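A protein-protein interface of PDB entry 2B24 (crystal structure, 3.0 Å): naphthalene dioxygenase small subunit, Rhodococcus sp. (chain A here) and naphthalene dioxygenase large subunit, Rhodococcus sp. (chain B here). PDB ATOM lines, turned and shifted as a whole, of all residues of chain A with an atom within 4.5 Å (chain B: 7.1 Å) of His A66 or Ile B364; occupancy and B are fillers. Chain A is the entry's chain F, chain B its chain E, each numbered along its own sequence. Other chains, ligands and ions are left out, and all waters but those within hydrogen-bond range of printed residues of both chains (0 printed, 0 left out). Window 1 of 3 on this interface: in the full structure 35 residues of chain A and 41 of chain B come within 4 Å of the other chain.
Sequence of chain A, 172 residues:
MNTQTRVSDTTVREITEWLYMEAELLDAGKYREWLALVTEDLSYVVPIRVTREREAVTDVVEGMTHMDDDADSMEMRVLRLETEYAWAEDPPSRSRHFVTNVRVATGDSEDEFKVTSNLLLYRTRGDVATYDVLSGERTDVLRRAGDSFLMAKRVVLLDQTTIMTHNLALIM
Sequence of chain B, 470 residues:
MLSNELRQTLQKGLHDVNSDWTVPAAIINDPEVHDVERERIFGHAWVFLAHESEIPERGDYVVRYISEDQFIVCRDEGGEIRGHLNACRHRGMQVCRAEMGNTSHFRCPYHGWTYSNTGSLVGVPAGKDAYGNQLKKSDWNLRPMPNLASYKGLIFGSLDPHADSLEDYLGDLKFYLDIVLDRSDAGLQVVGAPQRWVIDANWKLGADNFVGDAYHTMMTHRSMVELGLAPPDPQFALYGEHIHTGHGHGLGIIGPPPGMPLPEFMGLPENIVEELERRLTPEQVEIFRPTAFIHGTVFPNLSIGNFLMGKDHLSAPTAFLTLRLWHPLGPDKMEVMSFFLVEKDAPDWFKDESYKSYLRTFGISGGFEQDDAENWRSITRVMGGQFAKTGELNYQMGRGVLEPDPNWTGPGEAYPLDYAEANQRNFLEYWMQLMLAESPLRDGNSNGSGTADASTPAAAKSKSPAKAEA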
ATOM      1  N   VAL A  46      32.801   2.369  11.034  1.00  0.00           N
ATOM      2  CA  VAL A  46      31.634   2.828  10.262  1.00  0.00           C
ATOM      3  C   VAL A  46      30.993   4.025  10.988  1.00  0.00           C
ATOM      4  O   VAL A  46      30.177   3.827  11.867  1.00  0.00           O
ATOM      5  CB  VAL A  46      30.557   1.691  10.076  1.00  0.00           C
ATOM      6  CG1 VAL A  46      29.474   2.090   9.129  1.00  0.00           C
ATOM      7  CG2 VAL A  46      31.166   0.414   9.595  1.00  0.00           C
ATOM      8  N   PRO A  47      31.370   5.257  10.644  1.00  0.00           N
ATOM      9  CA  PRO A  47      30.847   6.453  11.322  1.00  0.00           C
ATOM     10  C   PRO A  47      29.345   6.662  11.214  1.00  0.00           C
ATOM     11  O   PRO A  47      28.733   6.156  10.287  1.00  0.00           O
ATOM     12  CB  PRO A  47      31.564   7.594  10.602  1.00  0.00           C
ATOM     13  CG  PRO A  47      32.783   6.983  10.020  1.00  0.00           C
ATOM     14  CD  PRO A  47      32.362   5.617   9.614  1.00  0.00           C
ATOM     15  N   ILE A  48      28.772   7.389  12.171  1.00  0.00           N
ATOM     16  CA  ILE A  48      27.363   7.776  12.151  1.00  0.00           C
ATOM     17  C   ILE A  48      27.306   9.110  11.427  1.00  0.00           C
ATOM     18  O   ILE A  48      28.238   9.871  11.475  1.00  0.00           O
ATOM     19  CB  ILE A  48      26.776   7.911  13.586  1.00  0.00           C
ATOM     20  CG1 ILE A  48      26.627   6.562  14.280  1.00  0.00           C
ATOM     21  CG2 ILE A  48      25.422   8.571  13.559  1.00  0.00           C
ATOM     22  CD1 ILE A  48      26.376   6.669  15.768  1.00  0.00           C
ATOM     23  N   THR A  65      29.803   5.692  16.767  1.00  0.00           N
ATOM     24  CA  THR A  65      30.076   4.916  15.578  1.00  0.00           C
ATOM     25  C   THR A  65      29.052   3.780  15.474  1.00  0.00           C
ATOM     26  O   THR A  65      28.423   3.424  16.463  1.00  0.00           O
ATOM     27  CB  THR A  65      31.492   4.348  15.699  1.00  0.00           C
ATOM     28  OG1 THR A  65      32.429   5.410  15.739  1.00  0.00           O
ATOM     29  CG2 THR A  65      31.926   3.707  14.439  1.00  0.00           C
ATOM     30  N   HIS A  66      28.879   3.231  14.271  1.00  0.00           N
ATOM     31  CA  HIS A  66      28.034   2.067  14.028  1.00  0.00           C
ATOM     32  C   HIS A  66      28.816   0.785  14.257  1.00  0.00           C
ATOM     33  O   HIS A  66      28.261  -0.250  14.593  1.00  0.00           O
ATOM     34  CB  HIS A  66      27.535   2.073  12.588  1.00  0.00           C
ATOM     35  CG  HIS A  66      26.413   3.031  12.324  1.00  0.00           C
ATOM     36  ND1 HIS A  66      25.186   2.936  12.943  1.00  0.00           N
ATOM     37  CD2 HIS A  66      26.324   4.080  11.478  1.00  0.00           C
ATOM     38  CE1 HIS A  66      24.397   3.896  12.504  1.00  0.00           C
ATOM     39  NE2 HIS A  66      25.069   4.606  11.617  1.00  0.00           N
ATOM     40  N   MET A  67      30.122   0.860  14.065  1.00  0.00           N
ATOM     41  CA  MET A  67      31.008  -0.282  14.150  1.00  0.00           C
ATOM     42  C   MET A  67      32.402   0.295  14.264  1.00  0.00           C
ATOM     43  O   MET A  67      32.779   1.109  13.445  1.00  0.00           O
ATOM     44  CB  MET A  67      30.896  -1.122  12.878  1.00  0.00           C
ATOM     45  CG  MET A  67      31.267  -2.571  13.047  1.00  0.00           C
ATOM     46  SD  MET A  67      31.612  -3.443  11.518  1.00  0.00           S
ATOM     47  CE  MET A  67      30.026  -3.935  10.973  1.00  0.00           C
ATOM     48  N   THR A 161      21.933   8.602   6.890  1.00  0.00           N
ATOM     49  CA  THR A 161      21.919   8.845   8.310  1.00  0.00           C
ATOM     50  C   THR A 161      21.159   7.695   9.009  1.00  0.00           C
ATOM     51  O   THR A 161      21.765   6.968   9.800  1.00  0.00           O
ATOM     52  CB  THR A 161      21.379  10.233   8.587  1.00  0.00           C
ATOM     53  OG1 THR A 161      20.128  10.404   7.927  1.00  0.00           O
ATOM     54  CG2 THR A 161      22.225  11.217   7.876  1.00  0.00           C
ATOM     55  N   ILE A 163      20.067   4.153   8.917  1.00  0.00           N
ATOM     56  CA  ILE A 163      20.584   3.005   8.167  1.00  0.00           C
ATOM     57  C   ILE A 163      19.453   2.090   7.703  1.00  0.00           C
ATOM     58  O   ILE A 163      18.627   1.658   8.502  1.00  0.00           O
ATOM     59  CB  ILE A 163      21.626   2.221   9.010  1.00  0.00           C
ATOM     60  CG1 ILE A 163      22.846   3.077   9.331  1.00  0.00           C
ATOM     61  CG2 ILE A 163      22.042   0.957   8.317  1.00  0.00           C
ATOM     62  CD1 ILE A 163      23.540   3.701   8.152  1.00  0.00           C
ATOM     63  N   ASN A 167      20.290  -4.895  10.732  1.00  0.00           N
ATOM     64  CA  ASN A 167      21.556  -4.976  11.464  1.00  0.00           C
ATOM     65  C   ASN A 167      22.752  -4.920  10.531  1.00  0.00           C
ATOM     66  O   ASN A 167      22.604  -5.075   9.318  1.00  0.00           O
ATOM     67  CB  ASN A 167      21.615  -6.217  12.353  1.00  0.00           C
ATOM     68  CG  ASN A 167      21.462  -7.517  11.576  1.00  0.00           C
ATOM     69  OD1 ASN A 167      21.966  -7.663  10.471  1.00  0.00           O
ATOM     70  ND2 ASN A 167      20.775  -8.480  12.174  1.00  0.00           N
ATOM     71  N   LEU A 168      23.932  -4.683  11.095  1.00  0.00           N
ATOM     72  CA  LEU A 168      25.168  -4.599  10.319  1.00  0.00           C
ATOM     73  C   LEU A 168      25.987  -5.868  10.504  1.00  0.00           C
ATOM     74  O   LEU A 168      27.124  -5.819  10.944  1.00  0.00           O
ATOM     75  CB  LEU A 168      25.961  -3.339  10.708  1.00  0.00           C
ATOM     76  CG  LEU A 168      26.072  -2.136   9.760  1.00  0.00           C
ATOM     77  CD1 LEU A 168      24.823  -1.881   8.949  1.00  0.00           C
ATOM     78  CD2 LEU A 168      26.422  -0.917  10.525  1.00  0.00           C
ATOM     79  N   PRO B 194      22.772   9.076  18.635  1.00  0.00           N
ATOM     80  CA  PRO B 194      22.251   7.710  18.682  1.00  0.00           C
ATOM     81  C   PRO B 194      22.538   6.951  17.376  1.00  0.00           C
ATOM     82  O   PRO B 194      22.675   7.590  16.343  1.00  0.00           O
ATOM     83  CB  PRO B 194      20.752   7.944  18.842  1.00  0.00           C
ATOM     84  CG  PRO B 194      20.513   9.225  18.186  1.00  0.00           C
ATOM     85  CD  PRO B 194      21.686  10.057  18.493  1.00  0.00           C
ATOM     86  N   GLN B 195      22.650   5.630  17.410  1.00  0.00           N
ATOM     87  CA  GLN B 195      22.591   4.875  16.169  1.00  0.00           C
ATOM     88  C   GLN B 195      21.138   4.782  15.764  1.00  0.00           C
ATOM     89  O   GLN B 195      20.306   4.375  16.542  1.00  0.00           O
ATOM     90  CB  GLN B 195      23.172   3.475  16.313  1.00  0.00           C
ATOM     91  CG  GLN B 195      24.559   3.468  16.874  1.00  0.00           C
ATOM     92  CD  GLN B 195      25.116   2.099  17.064  1.00  0.00           C
ATOM     93  OE1 GLN B 195      24.377   1.122  17.128  1.00  0.00           O
ATOM     94  NE2 GLN B 195      26.431   2.014  17.171  1.00  0.00           N
ATOM     95  N   ARG B 196      20.831   5.176  14.538  1.00  0.00           N
ATOM     96  CA  ARG B 196      19.474   5.129  14.039  1.00  0.00           C
ATOM     97  C   ARG B 196      19.441   4.171  12.860  1.00  0.00           C
ATOM     98  O   ARG B 196      20.144   4.395  11.869  1.00  0.00           O
ATOM     99  CB  ARG B 196      19.083   6.516  13.560  1.00  0.00           C
ATOM    100  CG  ARG B 196      18.572   7.463  14.601  1.00  0.00           C
ATOM    101  CD  ARG B 196      17.329   8.139  14.145  1.00  0.00           C
ATOM    102  NE  ARG B 196      17.467   9.575  14.014  1.00  0.00           N
ATOM    103  CZ  ARG B 196      16.538  10.374  13.479  1.00  0.00           C
ATOM    104  NH1 ARG B 196      15.398   9.888  13.016  1.00  0.00           N
ATOM    105  NH2 ARG B 196      16.744  11.683  13.406  1.00  0.00           N
ATOM    106  N   TRP B 197      18.640   3.111  12.974  1.00  0.00           N
ATOM    107  CA  TRP B 197      18.469   2.144  11.892  1.00  0.00           C
ATOM    108  C   TRP B 197      17.065   1.529  11.819  1.00  0.00           C
ATOM    109  O   TRP B 197      16.290   1.661  12.761  1.00  0.00           O
ATOM    110  CB  TRP B 197      19.566   1.078  11.937  1.00  0.00           C
ATOM    111  CG  TRP B 197      19.417  -0.032  12.921  1.00  0.00           C
ATOM    112  CD1 TRP B 197      18.981  -1.291  12.665  1.00  0.00           C
ATOM    113  CD2 TRP B 197      19.792  -0.013  14.301  1.00  0.00           C
ATOM    114  NE1 TRP B 197      19.032  -2.054  13.805  1.00  0.00           N
ATOM    115  CE2 TRP B 197      19.521  -1.286  14.827  1.00  0.00           C
ATOM    116  CE3 TRP B 197      20.314   0.958  15.155  1.00  0.00           C
ATOM    117  CZ2 TRP B 197      19.741  -1.603  16.166  1.00  0.00           C
ATOM    118  CZ3 TRP B 197      20.536   0.632  16.482  1.00  0.00           C
ATOM    119  CH2 TRP B 197      20.250  -0.631  16.972  1.00  0.00           C
ATOM    120  N   VAL B 198      16.744   0.863  10.710  1.00  0.00           N
ATOM    121  CA  VAL B 198      15.407   0.327  10.479  1.00  0.00           C
ATOM    122  C   VAL B 198      15.326  -1.208  10.525  1.00  0.00           C
ATOM    123  O   VAL B 198      15.842  -1.889   9.651  1.00  0.00           O
ATOM    124  CB  VAL B 198      14.841   0.839   9.137  1.00  0.00           C
ATOM    125  CG1 VAL B 198      13.530   0.175   8.809  1.00  0.00           C
ATOM    126  CG2 VAL B 198      14.654   2.331   9.164  1.00  0.00           C
ATOM    127  N   ARG B 324      17.435   3.311  24.575  1.00  0.00           N
ATOM    128  CA  ARG B 324      17.080   3.100  23.176  1.00  0.00           C
ATOM    129  C   ARG B 324      15.606   3.294  22.913  1.00  0.00           C
ATOM    130  O   ARG B 324      14.787   2.934  23.725  1.00  0.00           O
ATOM    131  CB  ARG B 324      17.483   1.700  22.732  1.00  0.00           C
ATOM    132  CG  ARG B 324      17.194   0.614  23.748  1.00  0.00           C
ATOM    133  CD  ARG B 324      18.407   0.130  24.532  1.00  0.00           C
ATOM    134  NE  ARG B 324      19.565  -0.064  23.687  1.00  0.00           N
ATOM    135  CZ  ARG B 324      19.702  -1.070  22.859  1.00  0.00           C
ATOM    136  NH1 ARG B 324      18.776  -2.000  22.777  1.00  0.00           N
ATOM    137  NH2 ARG B 324      20.777  -1.161  22.110  1.00  0.00           N
ATOM    138  N   VAL B 336      15.193   1.710  15.334  1.00  0.00           N
ATOM    139  CA  VAL B 336      15.880   1.752  16.620  1.00  0.00           C
ATOM    140  C   VAL B 336      16.693   3.025  16.705  1.00  0.00           C
ATOM    141  O   VAL B 336      17.378   3.400  15.761  1.00  0.00           O
ATOM    142  CB  VAL B 336      16.749   0.507  16.894  1.00  0.00           C
ATOM    143  CG1 VAL B 336      17.358   0.582  18.239  1.00  0.00           C
ATOM    144  CG2 VAL B 336      15.918  -0.744  16.840  1.00  0.00           C
ATOM    145  N   SER B 338      19.330   3.910  19.259  1.00  0.00           N
ATOM    146  CA  SER B 338      20.053   3.417  20.433  1.00  0.00           C
ATOM    147  C   SER B 338      21.128   4.357  20.947  1.00  0.00           C
ATOM    148  O   SER B 338      22.131   4.565  20.283  1.00  0.00           O
ATOM    149  CB  SER B 338      20.685   2.058  20.159  1.00  0.00           C
ATOM    150  OG  SER B 338      21.810   1.875  21.000  1.00  0.00           O
ATOM    151  N   TYR B 355      32.416   2.272  26.045  1.00  0.00           N
ATOM    152  CA  TYR B 355      31.838   2.501  24.724  1.00  0.00           C
ATOM    153  C   TYR B 355      32.068   1.309  23.814  1.00  0.00           C
ATOM    154  O   TYR B 355      31.193   0.957  23.033  1.00  0.00           O
ATOM    155  CB  TYR B 355      32.398   3.802  24.141  1.00  0.00           C
ATOM    156  CG  TYR B 355      32.627   3.847  22.640  1.00  0.00           C
ATOM    157  CD1 TYR B 355      31.556   3.916  21.739  1.00  0.00           C
ATOM    158  CD2 TYR B 355      33.917   3.872  22.122  1.00  0.00           C
ATOM    159  CE1 TYR B 355      31.777   3.974  20.382  1.00  0.00           C
ATOM    160  CE2 TYR B 355      34.133   3.934  20.768  1.00  0.00           C
ATOM    161  CZ  TYR B 355      33.063   3.983  19.904  1.00  0.00           C
ATOM    162  OH  TYR B 355      33.283   4.042  18.553  1.00  0.00           O
ATOM    163  N   TYR B 358      29.790  -1.575  24.663  1.00  0.00           N
ATOM    164  CA  TYR B 358      28.457  -1.331  24.104  1.00  0.00           C
ATOM    165  C   TYR B 358      28.452  -1.721  22.644  1.00  0.00           C
ATOM    166  O   TYR B 358      27.687  -2.588  22.232  1.00  0.00           O
ATOM    167  CB  TYR B 358      28.051   0.141  24.278  1.00  0.00           C
ATOM    168  CG  TYR B 358      26.971   0.633  23.351  1.00  0.00           C
ATOM    169  CD1 TYR B 358      25.649   0.325  23.562  1.00  0.00           C
ATOM    170  CD2 TYR B 358      27.278   1.432  22.274  1.00  0.00           C
ATOM    171  CE1 TYR B 358      24.671   0.789  22.709  1.00  0.00           C
ATOM    172  CE2 TYR B 358      26.305   1.900  21.423  1.00  0.00           C
ATOM    173  CZ  TYR B 358      25.015   1.568  21.644  1.00  0.00           C
ATOM    174  OH  TYR B 358      24.060   2.038  20.799  1.00  0.00           O
ATOM    175  N   LEU B 359      29.345  -1.097  21.881  1.00  0.00           N
ATOM    176  CA  LEU B 359      29.448  -1.276  20.443  1.00  0.00           C
ATOM    177  C   LEU B 359      29.501  -2.724  20.024  1.00  0.00           C
ATOM    178  O   LEU B 359      28.750  -3.137  19.164  1.00  0.00           O
ATOM    179  CB  LEU B 359      30.692  -0.579  19.931  1.00  0.00           C
ATOM    180  CG  LEU B 359      30.566   0.698  19.135  1.00  0.00           C
ATOM    181  CD1 LEU B 359      31.801   0.816  18.336  1.00  0.00           C
ATOM    182  CD2 LEU B 359      29.347   0.700  18.260  1.00  0.00           C
ATOM    183  N   THR B 361      28.791  -5.465  21.537  1.00  0.00           N
ATOM    184  CA  THR B 361      27.708  -6.327  21.990  1.00  0.00           C
ATOM    185  C   THR B 361      26.330  -5.813  21.546  1.00  0.00           C
ATOM    186  O   THR B 361      25.566  -6.547  20.915  1.00  0.00           O
ATOM    187  CB  THR B 361      27.738  -6.480  23.497  1.00  0.00           C
ATOM    188  OG1 THR B 361      27.646  -5.189  24.084  1.00  0.00           O
ATOM    189  CG2 THR B 361      29.077  -7.044  23.968  1.00  0.00           C
ATOM    190  N   PHE B 362      26.007  -4.562  21.859  1.00  0.00           N
ATOM    191  CA  PHE B 362      24.699  -4.031  21.486  1.00  0.00           C
ATOM    192  C   PHE B 362      24.784  -3.017  20.363  1.00  0.00           C
ATOM    193  O   PHE B 362      25.847  -2.767  19.849  1.00  0.00           O
ATOM    194  CB  PHE B 362      23.898  -3.563  22.724  1.00  0.00           C
ATOM    195  CG  PHE B 362      23.268  -4.709  23.471  1.00  0.00           C
ATOM    196  CD1 PHE B 362      24.044  -5.603  24.199  1.00  0.00           C
ATOM    197  CD2 PHE B 362      21.921  -4.946  23.383  1.00  0.00           C
ATOM    198  CE1 PHE B 362      23.475  -6.672  24.837  1.00  0.00           C
ATOM    199  CE2 PHE B 362      21.363  -6.027  24.021  1.00  0.00           C
ATOM    200  CZ  PHE B 362      22.148  -6.885  24.744  1.00  0.00           C
ATOM    201  N   GLY B 363      23.657  -2.483  19.935  1.00  0.00           N
ATOM    202  CA  GLY B 363      23.658  -1.575  18.811  1.00  0.00           C
ATOM    203  C   GLY B 363      23.529  -2.256  17.459  1.00  0.00           C
ATOM    204  O   GLY B 363      23.216  -3.447  17.368  1.00  0.00           O
ATOM    205  N   ILE B 364      23.774  -1.489  16.400  1.00  0.00           N
ATOM    206  CA  ILE B 364      23.525  -1.951  15.036  1.00  0.00           C
ATOM    207  C   ILE B 364      24.317  -3.215  14.683  1.00  0.00           C
ATOM    208  O   ILE B 364      23.748  -4.170  14.183  1.00  0.00           O
ATOM    209  CB  ILE B 364      23.670  -0.773  13.993  1.00  0.00           C
ATOM    210  CG1 ILE B 364      23.119  -1.169  12.626  1.00  0.00           C
ATOM    211  CG2 ILE B 364      25.085  -0.286  13.885  1.00  0.00           C
ATOM    212  CD1 ILE B 364      22.804  -0.022  11.751  1.00  0.00           C
ATOM    213  N   SER B 365      25.609  -3.212  15.003  1.00  0.00           N
ATOM    214  CA  SER B 365      26.571  -4.241  14.623  1.00  0.00           C
ATOM    215  C   SER B 365      26.996  -5.115  15.803  1.00  0.00           C
ATOM    216  O   SER B 365      27.994  -5.782  15.738  1.00  0.00           O
ATOM    217  CB  SER B 365      27.810  -3.561  14.042  1.00  0.00           C
ATOM    218  OG  SER B 365      28.529  -2.818  15.024  1.00  0.00           O
ATOM    219  N   GLY B 366      26.248  -5.111  16.891  1.00  0.00           N
ATOM    220  CA  GLY B 366      26.627  -5.876  18.058  1.00  0.00           C
ATOM    221  C   GLY B 366      26.545  -7.358  17.808  1.00  0.00           C
ATOM    222  O   GLY B 366      25.910  -7.786  16.861  1.00  0.00           O
ATOM    223  N   GLY B 367      27.198  -8.151  18.651  1.00  0.00           N
ATOM    224  CA  GLY B 367      27.132  -9.601  18.543  1.00  0.00           C
ATOM    225  C   GLY B 367      25.884 -10.120  19.219  1.00  0.00           C
ATOM    226  O   GLY B 367      25.385 -11.193  18.912  1.00  0.00           O
ATOM    227  N   GLU B 369      22.865  -7.815  19.941  1.00  0.00           N
ATOM    228  CA  GLU B 369      21.678  -7.201  19.380  1.00  0.00           C
ATOM    229  C   GLU B 369      21.369  -7.582  17.937  1.00  0.00           C
ATOM    230  O   GLU B 369      20.209  -7.529  17.553  1.00  0.00           O
ATOM    231  CB  GLU B 369      21.728  -5.686  19.524  1.00  0.00           C
ATOM    232  CG  GLU B 369      20.411  -4.984  19.236  1.00  0.00           C
ATOM    233  CD  GLU B 369      20.107  -3.885  20.230  1.00  0.00           C
ATOM    234  OE1 GLU B 369      20.674  -2.785  20.098  1.00  0.00           O
ATOM    235  OE2 GLU B 369      19.312  -4.116  21.148  1.00  0.00           O
ATOM    236  N   GLN B 370      22.369  -7.954  17.136  1.00  0.00           N
ATOM    237  CA  GLN B 370      22.114  -8.295  15.738  1.00  0.00           C
ATOM    238  C   GLN B 370      21.268  -9.574  15.582  1.00  0.00           C
ATOM    239  O   GLN B 370      20.539  -9.713  14.619  1.00  0.00           O
ATOM    240  CB  GLN B 370      23.414  -8.355  14.938  1.00  0.00           C
ATOM    241  CG  GLN B 370      24.212  -9.607  15.155  1.00  0.00           C
ATOM    242  CD  GLN B 370      25.500  -9.656  14.388  1.00  0.00           C
ATOM    243  OE1 GLN B 370      25.777 -10.641  13.700  1.00  0.00           O
ATOM    244  NE2 GLN B 370      26.314  -8.624  14.529  1.00  0.00           N
ATOM    245  N   ALA B 373      17.609  -8.555  16.602  1.00  0.00           N
ATOM    246  CA  ALA B 373      16.912  -7.936  15.481  1.00  0.00           C
ATOM    247  C   ALA B 373      16.424  -8.943  14.447  1.00  0.00           C
ATOM    248  O   ALA B 373      15.490  -8.654  13.716  1.00  0.00           O
ATOM    249  CB  ALA B 373      17.785  -6.894  14.834  1.00  0.00           C
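His A66 touches just these residues of chain B: Gln B195, Leu B359, Ile B364 and Ser B365.
Printed residues of chain A within 4 Å of Ile B364: His A66, Ile A163, Asn A167 and Leu A168.
Of the printed residues of chain B, Thr A161 touches Arg B196 (3.7 Å).
Of the printed residues of chain B, Leu A168 touches Ile B364 (3.1 Å) and Ser B365 (3.8 Å).
Of the printed residues of chain A, Ser B365 touches His A66, Met A67 and Leu A168.
Of the printed residues of chain B, Met A67 touches Ser B365.
Gly B363 touches none of the printed residues of chain A.
Gly B366 touches none of the printed residues of chain A.
The nearest residue of chain B that does not touch His A66 is Arg B196 (4.3 Å).
The nearest printed residue of chain A that does not touch Ile B364 is Met A67 (5.2 Å).
Pro B194 touches Ile A48 (O to CD1, 3.9 Å).
Ile A48 touches Gln B195 (CD1 to CG, 3.8 Å).
Leu B359 touches Thr A65.
CA of His A66 touches NE2 of Gln B195, at 3.5 Å.
His A66 touches Ile B364 (O to CG2, 3.3 Å).
Met A67 touches Ser B365.
Trp B197 touches Ile A163.
Ile A163 touches Ile B364 (CG2 to CD1, 3.7 Å).
Asn A167 touches Ile B364.
Leu A168 touches Ser B365.
The backbone NH of Ser B338 is in hydrogen-bond range of the backbone carbonyl oxygen of Gln B195 (2.9 Å).
The side-chain amide oxygen (OE1) of Gln B195 sits at hydrogen-bond distance from the backbone NH (N) of Ile B364, 2.8 Å away.
The backbone carbonyl oxygen (O) of Trp B197 sits at hydrogen-bond distance from the backbone NH (N) of Val B336, at 2.8 Å.
The side-chain amide nitrogen of Gln B370 lies within hydrogen-bond range of the backbone carbonyl oxygen of Gly B366, 2.5 Å away.
The backbone NH (N) of His A66 lies within hydrogen-bond range of the backbone carbonyl oxygen (O) of Val A46.
N of Val A46 is in hydrogen-bond range of O of Met A67 (2.7 Å).
The backbone carbonyl oxygen of Thr A65 is in hydrogen-bond range of the side-chain amide nitrogen of Gln B195 (2.5 Å).
The backbone carbonyl oxygen (O) of Arg B196 sits at hydrogen-bond distance from the backbone NH (N) of Ile A163.
N of Val B198 lies within hydrogen-bond range of O of Ile A163, at 3.0 Å.
The side-chain hydroxyl (OG1) of Thr A65 is in hydrogen-bond range of the side-chain hydroxyl (OH) of Tyr B355 (3.2 Å).
The backbone carbonyl oxygen of Ile B364 is in hydrogen-bond range of the backbone NH of Leu A168 (3.1 Å).
The backbone carbonyl oxygen of His A66 sits at hydrogen-bond distance from the side-chain hydroxyl of Ser B365 (2.6 Å).
The side-chain amide nitrogen (ND2) of Asn A167 sits at hydrogen-bond distance from the backbone carbonyl oxygen (O) of Gln B370, at 2.7 Å.
Hydrophobic or aromatic side chains of chain A that line the printed part of chain B: Ile A48, His A66, Met A67, Ile A163 and Leu A168.
Among the printed residues, 19 pairs touch across the chains.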
